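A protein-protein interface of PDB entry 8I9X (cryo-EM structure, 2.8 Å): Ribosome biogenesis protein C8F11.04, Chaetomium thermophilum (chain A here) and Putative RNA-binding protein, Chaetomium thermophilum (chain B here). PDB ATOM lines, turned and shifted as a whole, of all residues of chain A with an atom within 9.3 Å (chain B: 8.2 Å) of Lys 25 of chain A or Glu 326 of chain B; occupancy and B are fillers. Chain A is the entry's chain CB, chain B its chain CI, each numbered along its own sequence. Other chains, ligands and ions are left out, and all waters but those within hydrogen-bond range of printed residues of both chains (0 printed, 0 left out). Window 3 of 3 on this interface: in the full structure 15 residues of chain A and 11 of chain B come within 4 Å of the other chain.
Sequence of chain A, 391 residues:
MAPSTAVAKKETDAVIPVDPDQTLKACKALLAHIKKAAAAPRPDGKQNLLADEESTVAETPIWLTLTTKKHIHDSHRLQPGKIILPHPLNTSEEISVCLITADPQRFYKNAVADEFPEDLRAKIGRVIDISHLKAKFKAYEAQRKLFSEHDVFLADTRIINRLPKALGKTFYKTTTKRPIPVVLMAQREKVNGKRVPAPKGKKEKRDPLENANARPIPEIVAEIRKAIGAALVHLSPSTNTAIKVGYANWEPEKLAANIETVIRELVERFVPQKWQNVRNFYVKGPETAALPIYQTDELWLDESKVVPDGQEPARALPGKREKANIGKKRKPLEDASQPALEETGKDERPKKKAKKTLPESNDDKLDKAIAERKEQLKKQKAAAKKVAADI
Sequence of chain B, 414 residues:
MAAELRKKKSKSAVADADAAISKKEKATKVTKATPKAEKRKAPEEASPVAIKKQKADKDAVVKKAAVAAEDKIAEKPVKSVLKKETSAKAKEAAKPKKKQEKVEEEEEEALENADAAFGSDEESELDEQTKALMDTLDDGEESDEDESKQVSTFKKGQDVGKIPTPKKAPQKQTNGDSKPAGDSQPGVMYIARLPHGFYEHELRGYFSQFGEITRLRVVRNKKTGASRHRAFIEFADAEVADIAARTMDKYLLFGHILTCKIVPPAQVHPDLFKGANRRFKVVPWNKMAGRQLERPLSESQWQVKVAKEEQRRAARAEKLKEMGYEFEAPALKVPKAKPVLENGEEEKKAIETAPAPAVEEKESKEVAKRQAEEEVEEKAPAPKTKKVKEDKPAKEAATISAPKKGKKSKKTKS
The backbone carbonyl oxygen of Val 283 of chain A sits at hydrogen-bond distance from the backbone NH of Leu 291 of chain A, 2.8 Å away.
The side-chain carboxylate of Asp 21 of chain A lies close to the side-chain amide oxygen of Gln 22 of chain A.
The backbone carbonyl oxygen (O) of Leu 320 of chain B sits at hydrogen-bond distance from the backbone NH (N) of Tyr 325 of chain B (3.4 Å).
OE1 of Gln 22 of chain A sits close to O of Asp 19 of chain A (3.1 Å).
Gln 22 of chain A touches Tyr 325 of chain B (O to CE1, 3.7 Å).
Tyr 325 of chain B touches Ala 26 of chain A.
CD2 of Leu 291 of chain A touches CD2 of Leu 320 of chain B, at 3.6 Å.
Tyr 325 of chain B touches Leu 291 of chain A (CD2 to CD2, 3.5 Å).
CD1 of Leu 320 of chain B touches CD of Pro 292 of chain A (3.9 Å).
Pro 292 of chain A touches Phe 327 of chain B (CB to CD2, 3.8 Å).
Ile 293 of chain A touches Tyr 325 of chain B.
Phe 327 of chain B touches Ile 293 of chain A (CZ to C, 3.8 Å).
Of chain B, only Glu 326 comes within 4 Å of Lys 25 of chain A.
Ala 26 of chain A touches just one residue of chain B: Tyr 325 (3.5 Å).
Of the printed residues of chain B, His 33 of chain A touches Met 323.
Of the printed residues of chain A, Leu 320 of chain B touches Leu 291 and Pro 292.
Tyr 325 of chain B touches five residues of chain A.
Glu 326 of chain B touches just one residue of chain A: Lys 25.
The nearest residue of chain B that does not touch Lys 25 of chain A is Tyr 325 of chain B (4.2 Å).
The nearest residue of chain A that does not touch Glu 326 of chain B is Gln 22 of chain A (5.2 Å).
The nearest printed residue of chain A that does not touch Met 323 of chain B is Ala 29 of chain A (4.02 Å).
Of the 11 printed residues of chain B, 5 touch a printed residue of chain A.
Hydrophobic or aromatic side chains of chain B within 4 Å of the printed part of chain A: Leu 320, Met 323, Tyr 325 and Phe 327.
Of the 23 printed residues of chain A, 7 touch a printed residue of chain B.
Hydrophobic or aromatic side chains of chain A within 4 Å of the printed part of chain B: Ala 26, His 33, Leu 291, Pro 292 and Ile 293.
Among the printed residues, 11 pairs touch across the chains.
Among the printed residues, Asp or Glu carboxylates within 4 Å of a Lys or Arg side-chain nitrogen of the other chain: Lys 25 of chain A with Glu 326 of chain B (3.4 Å).
The side-chain hydroxyl (OH) of Tyr 325 of chain B sits at hydrogen-bond distance from the backbone carbonyl oxygen (O) of Pro 292 of chain A.
The side-chain carboxylate (OE1) of Glu 326 of chain B lies within salt-bridge range of the side-chain amino group (NZ) of Lys 25 of chain A (3.4 Å).
SD of Met 323 of chain B sits at hydrogen-bond distance from ND1 of His 33 of chain A (3.0 Å).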
ATOM      1  N   ASP A  19     -11.923  -2.965  15.573  1.00  0.00           N
ATOM      2  CA  ASP A  19     -11.335  -4.004  16.408  1.00  0.00           C
ATOM      3  C   ASP A  19     -10.425  -4.897  15.567  1.00  0.00           C
ATOM      4  O   ASP A  19     -10.862  -5.504  14.568  1.00  0.00           O
ATOM      5  CB  ASP A  19     -12.435  -4.809  17.103  1.00  0.00           C
ATOM      6  CG  ASP A  19     -11.962  -5.502  18.371  1.00  0.00           C
ATOM      7  OD1 ASP A  19     -10.805  -5.302  18.783  1.00  0.00           O
ATOM      8  OD2 ASP A  19     -12.762  -6.259  18.959  1.00  0.00           O
ATOM      9  N   PRO A  20      -9.148  -4.995  15.953  1.00  0.00           N
ATOM     10  CA  PRO A  20      -8.168  -5.696  15.115  1.00  0.00           C
ATOM     11  C   PRO A  20      -8.525  -7.134  14.800  1.00  0.00           C
ATOM     12  O   PRO A  20      -8.151  -7.605  13.724  1.00  0.00           O
ATOM     13  CB  PRO A  20      -6.873  -5.614  15.940  1.00  0.00           C
ATOM     14  CG  PRO A  20      -7.300  -5.201  17.318  1.00  0.00           C
ATOM     15  CD  PRO A  20      -8.508  -4.353  17.110  1.00  0.00           C
ATOM     16  N   ASP A  21      -9.234  -7.846  15.678  1.00  0.00           N
ATOM     17  CA  ASP A  21      -9.548  -9.241  15.378  1.00  0.00           C
ATOM     18  C   ASP A  21     -10.447  -9.376  14.148  1.00  0.00           C
ATOM     19  O   ASP A  21     -10.111 -10.127  13.219  1.00  0.00           O
ATOM     20  CB  ASP A  21     -10.152  -9.933  16.606  1.00  0.00           C
ATOM     21  CG  ASP A  21     -11.268  -9.140  17.236  1.00  0.00           C
ATOM     22  OD1 ASP A  21     -11.531  -8.029  16.749  1.00  0.00           O
ATOM     23  OD2 ASP A  21     -11.883  -9.624  18.211  1.00  0.00           O
ATOM     24  N   GLN A  22     -11.577  -8.655  14.088  1.00  0.00           N
ATOM     25  CA  GLN A  22     -12.390  -8.819  12.885  1.00  0.00           C
ATOM     26  C   GLN A  22     -11.780  -8.095  11.695  1.00  0.00           C
ATOM     27  O   GLN A  22     -11.987  -8.523  10.555  1.00  0.00           O
ATOM     28  CB  GLN A  22     -13.851  -8.371  13.044  1.00  0.00           C
ATOM     29  CG  GLN A  22     -14.128  -6.886  13.180  1.00  0.00           C
ATOM     30  CD  GLN A  22     -14.010  -6.395  14.585  1.00  0.00           C
ATOM     31  OE1 GLN A  22     -13.440  -7.065  15.432  1.00  0.00           O
ATOM     32  NE2 GLN A  22     -14.578  -5.225  14.855  1.00  0.00           N
ATOM     33  N   THR A  23     -11.017  -7.016  11.917  1.00  0.00           N
ATOM     34  CA  THR A  23     -10.333  -6.430  10.765  1.00  0.00           C
ATOM     35  C   THR A  23      -9.367  -7.433  10.142  1.00  0.00           C
ATOM     36  O   THR A  23      -9.323  -7.583   8.917  1.00  0.00           O
ATOM     37  CB  THR A  23      -9.592  -5.152  11.153  1.00  0.00           C
ATOM     38  OG1 THR A  23      -8.585  -5.457  12.122  1.00  0.00           O
ATOM     39  CG2 THR A  23     -10.557  -4.120  11.717  1.00  0.00           C
ATOM     40  N   LEU A  24      -8.611  -8.152  10.974  1.00  0.00           N
ATOM     41  CA  LEU A  24      -7.656  -9.129  10.471  1.00  0.00           C
ATOM     42  C   LEU A  24      -8.361 -10.309   9.815  1.00  0.00           C
ATOM     43  O   LEU A  24      -7.894 -10.824   8.790  1.00  0.00           O
ATOM     44  CB  LEU A  24      -6.756  -9.604  11.610  1.00  0.00           C
ATOM     45  CG  LEU A  24      -5.721 -10.681  11.287  1.00  0.00           C
ATOM     46  CD1 LEU A  24      -4.785 -10.192  10.197  1.00  0.00           C
ATOM     47  CD2 LEU A  24      -4.944 -11.070  12.535  1.00  0.00           C
ATOM     48  N   LYS A  25      -9.475 -10.766  10.394  1.00  0.00           N
ATOM     49  CA  LYS A  25     -10.185 -11.874   9.762  1.00  0.00           C
ATOM     50  C   LYS A  25     -10.796 -11.466   8.427  1.00  0.00           C
ATOM     51  O   LYS A  25     -10.751 -12.254   7.477  1.00  0.00           O
ATOM     52  CB  LYS A  25     -11.251 -12.452  10.701  1.00  0.00           C
ATOM     53  CG  LYS A  25     -12.537 -11.661  10.819  1.00  0.00           C
ATOM     54  CD  LYS A  25     -13.435 -12.241  11.900  1.00  0.00           C
ATOM     55  CE  LYS A  25     -14.460 -13.195  11.310  1.00  0.00           C
ATOM     56  NZ  LYS A  25     -15.488 -13.599  12.308  1.00  0.00           N
ATOM     57  N   ALA A  26     -11.330 -10.246   8.320  1.00  0.00           N
ATOM     58  CA  ALA A  26     -11.794  -9.761   7.026  1.00  0.00           C
ATOM     59  C   ALA A  26     -10.639  -9.657   6.041  1.00  0.00           C
ATOM     60  O   ALA A  26     -10.786 -10.002   4.862  1.00  0.00           O
ATOM     61  CB  ALA A  26     -12.485  -8.408   7.187  1.00  0.00           C
ATOM     62  N   CYS A  27      -9.482  -9.184   6.507  1.00  0.00           N
ATOM     63  CA  CYS A  27      -8.320  -9.086   5.634  1.00  0.00           C
ATOM     64  C   CYS A  27      -7.947 -10.448   5.067  1.00  0.00           C
ATOM     65  O   CYS A  27      -7.823 -10.608   3.848  1.00  0.00           O
ATOM     66  CB  CYS A  27      -7.145  -8.474   6.396  1.00  0.00           C
ATOM     67  SG  CYS A  27      -5.638  -8.280   5.418  1.00  0.00           S
ATOM     68  N   LYS A  28      -7.787 -11.451   5.933  1.00  0.00           N
ATOM     69  CA  LYS A  28      -7.420 -12.769   5.429  1.00  0.00           C
ATOM     70  C   LYS A  28      -8.518 -13.385   4.572  1.00  0.00           C
ATOM     71  O   LYS A  28      -8.206 -14.122   3.631  1.00  0.00           O
ATOM     72  CB  LYS A  28      -7.047 -13.722   6.570  1.00  0.00           C
ATOM     73  CG  LYS A  28      -8.164 -14.083   7.529  1.00  0.00           C
ATOM     74  CD  LYS A  28      -7.665 -15.069   8.579  1.00  0.00           C
ATOM     75  CE  LYS A  28      -6.728 -14.417   9.584  1.00  0.00           C
ATOM     76  NZ  LYS A  28      -7.409 -13.404  10.430  1.00  0.00           N
ATOM     77  N   ALA A  29      -9.789 -13.087   4.852  1.00  0.00           N
ATOM     78  CA  ALA A  29     -10.856 -13.567   3.980  1.00  0.00           C
ATOM     79  C   ALA A  29     -10.730 -12.974   2.583  1.00  0.00           C
ATOM     80  O   ALA A  29     -10.890 -13.685   1.580  1.00  0.00           O
ATOM     81  CB  ALA A  29     -12.219 -13.234   4.585  1.00  0.00           C
ATOM     82  N   LEU A  30     -10.440 -11.676   2.498  1.00  0.00           N
ATOM     83  CA  LEU A  30     -10.258 -11.052   1.191  1.00  0.00           C
ATOM     84  C   LEU A  30      -9.048 -11.634   0.474  1.00  0.00           C
ATOM     85  O   LEU A  30      -9.094 -11.866  -0.738  1.00  0.00           O
ATOM     86  CB  LEU A  30     -10.132  -9.534   1.340  1.00  0.00           C
ATOM     87  CG  LEU A  30     -10.112  -8.671   0.072  1.00  0.00           C
ATOM     88  CD1 LEU A  30     -10.639  -7.284   0.380  1.00  0.00           C
ATOM     89  CD2 LEU A  30      -8.713  -8.557  -0.514  1.00  0.00           C
ATOM     90  N   LEU A  31      -7.955 -11.868   1.204  1.00  0.00           N
ATOM     91  CA  LEU A  31      -6.788 -12.496   0.590  1.00  0.00           C
ATOM     92  C   LEU A  31      -7.118 -13.881   0.048  1.00  0.00           C
ATOM     93  O   LEU A  31      -6.688 -14.239  -1.055  1.00  0.00           O
ATOM     94  CB  LEU A  31      -5.628 -12.567   1.585  1.00  0.00           C
ATOM     95  CG  LEU A  31      -4.726 -11.341   1.756  1.00  0.00           C
ATOM     96  CD1 LEU A  31      -4.025 -11.107   0.446  1.00  0.00           C
ATOM     97  CD2 LEU A  31      -5.448 -10.077   2.162  1.00  0.00           C
ATOM     98  N   ALA A  32      -7.882 -14.672   0.804  1.00  0.00           N
ATOM     99  CA  ALA A  32      -8.283 -15.988   0.319  1.00  0.00           C
ATOM    100  C   ALA A  32      -9.144 -15.885  -0.932  1.00  0.00           C
ATOM    101  O   ALA A  32      -8.965 -16.671  -1.875  1.00  0.00           O
ATOM    102  CB  ALA A  32      -9.025 -16.750   1.415  1.00  0.00           C
ATOM    103  N   HIS A  33     -10.082 -14.935  -0.959  1.00  0.00           N
ATOM    104  CA  HIS A  33     -10.919 -14.776  -2.144  1.00  0.00           C
ATOM    105  C   HIS A  33     -10.078 -14.376  -3.352  1.00  0.00           C
ATOM    106  O   HIS A  33     -10.274 -14.897  -4.455  1.00  0.00           O
ATOM    107  CB  HIS A  33     -12.029 -13.757  -1.881  1.00  0.00           C
ATOM    108  CG  HIS A  33     -12.991 -13.598  -3.021  1.00  0.00           C
ATOM    109  ND1 HIS A  33     -14.356 -13.549  -2.836  1.00  0.00           N
ATOM    110  CD2 HIS A  33     -12.790 -13.455  -4.353  1.00  0.00           C
ATOM    111  CE1 HIS A  33     -14.953 -13.403  -4.005  1.00  0.00           C
ATOM    112  NE2 HIS A  33     -14.025 -13.340  -4.941  1.00  0.00           N
ATOM    113  N   PRO A 252      -1.334 -10.723   6.142  1.00  0.00           N
ATOM    114  CA  PRO A 252      -2.541 -10.080   6.677  1.00  0.00           C
ATOM    115  C   PRO A 252      -2.258  -9.174   7.860  1.00  0.00           C
ATOM    116  O   PRO A 252      -2.901  -8.128   7.986  1.00  0.00           O
ATOM    117  CB  PRO A 252      -3.435 -11.271   7.058  1.00  0.00           C
ATOM    118  CG  PRO A 252      -2.533 -12.450   7.098  1.00  0.00           C
ATOM    119  CD  PRO A 252      -1.479 -12.185   6.081  1.00  0.00           C
ATOM    120  N   GLU A 253      -1.302  -9.528   8.721  1.00  0.00           N
ATOM    121  CA  GLU A 253      -0.933  -8.636   9.819  1.00  0.00           C
ATOM    122  C   GLU A 253      -0.268  -7.367   9.308  1.00  0.00           C
ATOM    123  O   GLU A 253      -0.512  -6.278   9.846  1.00  0.00           O
ATOM    124  CB  GLU A 253      -0.018  -9.363  10.806  1.00  0.00           C
ATOM    125  CG  GLU A 253      -0.727 -10.412  11.657  1.00  0.00           C
ATOM    126  CD  GLU A 253      -0.811 -11.772  10.979  1.00  0.00           C
ATOM    127  OE1 GLU A 253      -0.274 -11.911   9.857  1.00  0.00           O
ATOM    128  OE2 GLU A 253      -1.415 -12.699  11.569  1.00  0.00           O
ATOM    129  N   ALA A 256      -3.048  -5.280   8.060  1.00  0.00           N
ATOM    130  CA  ALA A 256      -3.851  -4.777   9.165  1.00  0.00           C
ATOM    131  C   ALA A 256      -3.174  -3.601   9.859  1.00  0.00           C
ATOM    132  O   ALA A 256      -3.838  -2.622  10.225  1.00  0.00           O
ATOM    133  CB  ALA A 256      -4.134  -5.903  10.159  1.00  0.00           C
ATOM    134  N   ILE A 259      -3.662  -0.674   7.671  1.00  0.00           N
ATOM    135  CA  ILE A 259      -5.034  -0.192   7.773  1.00  0.00           C
ATOM    136  C   ILE A 259      -5.265   0.617   9.039  1.00  0.00           C
ATOM    137  O   ILE A 259      -5.860   1.700   8.972  1.00  0.00           O
ATOM    138  CB  ILE A 259      -6.026  -1.366   7.713  1.00  0.00           C
ATOM    139  CG1 ILE A 259      -6.033  -1.977   6.313  1.00  0.00           C
ATOM    140  CG2 ILE A 259      -7.426  -0.908   8.094  1.00  0.00           C
ATOM    141  CD1 ILE A 259      -6.739  -3.305   6.232  1.00  0.00           C
ATOM    142  N   VAL A 283     -13.329  -2.470   3.240  1.00  0.00           N
ATOM    143  CA  VAL A 283     -12.083  -2.876   2.522  1.00  0.00           C
ATOM    144  C   VAL A 283     -12.521  -3.363   1.142  1.00  0.00           C
ATOM    145  O   VAL A 283     -13.618  -3.943   1.061  1.00  0.00           O
ATOM    146  CB  VAL A 283     -11.268  -3.937   3.282  1.00  0.00           C
ATOM    147  CG1 VAL A 283      -9.934  -4.238   2.622  1.00  0.00           C
ATOM    148  CG2 VAL A 283     -11.061  -3.550   4.736  1.00  0.00           C
ATOM    149  N   LEU A 291     -15.866  -5.301   2.160  1.00  0.00           N
ATOM    150  CA  LEU A 291     -15.856  -5.854   3.514  1.00  0.00           C
ATOM    151  C   LEU A 291     -16.202  -4.739   4.488  1.00  0.00           C
ATOM    152  O   LEU A 291     -15.402  -3.803   4.668  1.00  0.00           O
ATOM    153  CB  LEU A 291     -14.490  -6.447   3.845  1.00  0.00           C
ATOM    154  CG  LEU A 291     -14.074  -7.667   3.028  1.00  0.00           C
ATOM    155  CD1 LEU A 291     -12.655  -8.047   3.374  1.00  0.00           C
ATOM    156  CD2 LEU A 291     -15.022  -8.830   3.263  1.00  0.00           C
ATOM    157  N   PRO A 292     -17.302  -4.779   5.265  1.00  0.00           N
ATOM    158  CA  PRO A 292     -17.519  -3.731   6.257  1.00  0.00           C
ATOM    159  C   PRO A 292     -16.510  -3.644   7.414  1.00  0.00           C
ATOM    160  O   PRO A 292     -15.891  -4.631   7.689  1.00  0.00           O
ATOM    161  CB  PRO A 292     -18.902  -4.079   6.834  1.00  0.00           C
ATOM    162  CG  PRO A 292     -19.567  -4.885   5.754  1.00  0.00           C
ATOM    163  CD  PRO A 292     -18.434  -5.726   5.217  1.00  0.00           C
ATOM    164  N   ILE A 293     -16.340  -2.462   8.020  1.00  0.00           N
ATOM    165  CA  ILE A 293     -15.521  -2.242   9.253  1.00  0.00           C
ATOM    166  C   ILE A 293     -16.233  -1.065   9.932  1.00  0.00           C
ATOM    167  O   ILE A 293     -15.615  -0.392  10.769  1.00  0.00           O
ATOM    168  CB  ILE A 293     -14.037  -1.937   8.952  1.00  0.00           C
ATOM    169  CG1 ILE A 293     -13.437  -2.811   7.846  1.00  0.00           C
ATOM    170  CG2 ILE A 293     -13.193  -2.029  10.217  1.00  0.00           C
ATOM    171  CD1 ILE A 293     -12.776  -4.076   8.344  1.00  0.00           C
ATOM    172  N   ALA B 317     -24.630  -9.669   3.576  1.00  0.00           N
ATOM    173  CA  ALA B 317     -24.336 -10.890   4.310  1.00  0.00           C
ATOM    174  C   ALA B 317     -24.412 -12.109   3.404  1.00  0.00           C
ATOM    175  O   ALA B 317     -23.587 -13.022   3.519  1.00  0.00           O
ATOM    176  CB  ALA B 317     -25.297 -11.033   5.489  1.00  0.00           C
ATOM    177  N   LEU B 320     -21.466 -12.190   1.431  1.00  0.00           N
ATOM    178  CA  LEU B 320     -20.324 -12.435   2.303  1.00  0.00           C
ATOM    179  C   LEU B 320     -20.292 -13.850   2.868  1.00  0.00           C
ATOM    180  O   LEU B 320     -19.295 -14.222   3.496  1.00  0.00           O
ATOM    181  CB  LEU B 320     -20.311 -11.435   3.467  1.00  0.00           C
ATOM    182  CG  LEU B 320     -19.890  -9.980   3.234  1.00  0.00           C
ATOM    183  CD1 LEU B 320     -20.046  -9.181   4.518  1.00  0.00           C
ATOM    184  CD2 LEU B 320     -18.467  -9.883   2.725  1.00  0.00           C
ATOM    185  N   LYS B 321     -21.350 -14.634   2.684  1.00  0.00           N
ATOM    186  CA  LYS B 321     -21.306 -16.032   3.097  1.00  0.00           C
ATOM    187  C   LYS B 321     -20.280 -16.810   2.288  1.00  0.00           C
ATOM    188  O   LYS B 321     -19.576 -17.666   2.836  1.00  0.00           O
ATOM    189  CB  LYS B 321     -22.687 -16.680   2.961  1.00  0.00           C
ATOM    190  CG  LYS B 321     -23.762 -16.116   3.887  1.00  0.00           C
ATOM    191  CD  LYS B 321     -23.445 -16.349   5.362  1.00  0.00           C
ATOM    192  CE  LYS B 321     -22.946 -15.081   6.044  1.00  0.00           C
ATOM    193  NZ  LYS B 321     -22.742 -15.279   7.505  1.00  0.00           N
ATOM    194  N   GLU B 322     -20.188 -16.525   0.988  1.00  0.00           N
ATOM    195  CA  GLU B 322     -19.091 -17.059   0.192  1.00  0.00           C
ATOM    196  C   GLU B 322     -17.764 -16.472   0.649  1.00  0.00           C
ATOM    197  O   GLU B 322     -16.724 -17.138   0.591  1.00  0.00           O
ATOM    198  CB  GLU B 322     -19.325 -16.769  -1.292  1.00  0.00           C
ATOM    199  CG  GLU B 322     -20.569 -17.424  -1.882  1.00  0.00           C
ATOM    200  CD  GLU B 322     -21.851 -16.710  -1.495  1.00  0.00           C
ATOM    201  OE1 GLU B 322     -22.003 -15.523  -1.851  1.00  0.00           O
ATOM    202  OE2 GLU B 322     -22.706 -17.336  -0.832  1.00  0.00           O
ATOM    203  N   MET B 323     -17.783 -15.220   1.111  1.00  0.00           N
ATOM    204  CA  MET B 323     -16.592 -14.577   1.648  1.00  0.00           C
ATOM    205  C   MET B 323     -16.226 -15.213   2.981  1.00  0.00           C
ATOM    206  O   MET B 323     -15.096 -15.669   3.176  1.00  0.00           O
ATOM    207  CB  MET B 323     -16.822 -13.078   1.844  1.00  0.00           C
ATOM    208  CG  MET B 323     -17.066 -12.267   0.583  1.00  0.00           C
ATOM    209  SD  MET B 323     -15.723 -12.181  -0.606  1.00  0.00           S
ATOM    210  CE  MET B 323     -16.576 -11.349  -1.944  1.00  0.00           C
ATOM    211  N   GLY B 324     -17.188 -15.247   3.901  1.00  0.00           N
ATOM    212  CA  GLY B 324     -16.968 -15.807   5.220  1.00  0.00           C
ATOM    213  C   GLY B 324     -16.750 -14.754   6.285  1.00  0.00           C
ATOM    214  O   GLY B 324     -16.252 -15.057   7.373  1.00  0.00           O
ATOM    215  N   TYR B 325     -17.124 -13.512   5.989  1.00  0.00           N
ATOM    216  CA  TYR B 325     -16.912 -12.391   6.900  1.00  0.00           C
ATOM    217  C   TYR B 325     -18.246 -12.032   7.546  1.00  0.00           C
ATOM    218  O   TYR B 325     -19.194 -11.639   6.863  1.00  0.00           O
ATOM    219  CB  TYR B 325     -16.306 -11.203   6.162  1.00  0.00           C
ATOM    220  CG  TYR B 325     -16.053 -10.003   7.045  1.00  0.00           C
ATOM    221  CD1 TYR B 325     -15.609 -10.160   8.351  1.00  0.00           C
ATOM    222  CD2 TYR B 325     -16.257  -8.713   6.573  1.00  0.00           C
ATOM    223  CE1 TYR B 325     -15.377  -9.068   9.162  1.00  0.00           C
ATOM    224  CE2 TYR B 325     -16.026  -7.615   7.376  1.00  0.00           C
ATOM    225  CZ  TYR B 325     -15.587  -7.798   8.669  1.00  0.00           C
ATOM    226  OH  TYR B 325     -15.356  -6.707   9.475  1.00  0.00           O
ATOM    227  N   GLU B 326     -18.316 -12.175   8.867  1.00  0.00           N
ATOM    228  CA  GLU B 326     -19.509 -11.805   9.614  1.00  0.00           C
ATOM    229  C   GLU B 326     -19.250 -10.529  10.405  1.00  0.00           C
ATOM    230  O   GLU B 326     -18.216 -10.401  11.069  1.00  0.00           O
ATOM    231  CB  GLU B 326     -19.929 -12.936  10.551  1.00  0.00           C
ATOM    232  CG  GLU B 326     -20.197 -14.262   9.857  1.00  0.00           C
ATOM    233  CD  GLU B 326     -18.947 -15.106   9.702  1.00  0.00           C
ATOM    234  OE1 GLU B 326     -17.890 -14.709  10.236  1.00  0.00           O
ATOM    235  OE2 GLU B 326     -19.021 -16.166   9.047  1.00  0.00           O
ATOM    236  N   PHE B 327     -20.188  -9.587  10.333  1.00  0.00           N
ATOM    237  CA  PHE B 327     -20.069  -8.310  11.020  1.00  0.00           C
ATOM    238  C   PHE B 327     -21.352  -8.014  11.783  1.00  0.00           C
ATOM    239  O   PHE B 327     -22.444  -8.387  11.346  1.00  0.00           O
ATOM    240  CB  PHE B 327     -19.774  -7.173  10.034  1.00  0.00           C
ATOM    241  CG  PHE B 327     -19.202  -5.945  10.681  1.00  0.00           C
ATOM    242  CD1 PHE B 327     -18.058  -6.024  11.457  1.00  0.00           C
ATOM    243  CD2 PHE B 327     -19.809  -4.712  10.517  1.00  0.00           C
ATOM    244  CE1 PHE B 327     -17.529  -4.897  12.056  1.00  0.00           C
ATOM    245  CE2 PHE B 327     -19.286  -3.581  11.113  1.00  0.00           C
ATOM    246  CZ  PHE B 327     -18.144  -3.673  11.883  1.00  0.00           C
ATOM    247  N   GLU B 328     -21.211  -7.343  12.925  1.00  0.00           N
ATOM    248  CA  GLU B 328     -22.362  -7.001  13.753  1.00  0.00           C
ATOM    249  C   GLU B 328     -22.900  -5.621  13.394  1.00  0.00           C
ATOM    250  O   GLU B 328     -22.466  -5.017  12.407  1.00  0.00           O
ATOM    251  CB  GLU B 328     -21.990  -7.069  15.236  1.00  0.00           C
ATOM    252  CG  GLU B 328     -20.862  -6.138  15.650  1.00  0.00           C
ATOM    253  CD  GLU B 328     -21.365  -4.813  16.188  1.00  0.00           C
ATOM    254  OE1 GLU B 328     -22.541  -4.749  16.604  1.00  0.00           O
ATOM    255  OE2 GLU B 328     -20.586  -3.838  16.195  1.00  0.00           O
ATOM    256  N   ALA B 329     -23.841  -5.115  14.186  1.00  0.00           N
ATOM    257  CA  ALA B 329     -24.481  -3.834  13.898  1.00  0.00           C
ATOM    258  C   ALA B 329     -23.894  -2.704  14.738  1.00  0.00           C
ATOM    259  O   ALA B 329     -24.615  -1.994  15.440  1.00  0.00           O
ATOM    260  CB  ALA B 329     -25.981  -3.935  14.125  1.00  0.00           C
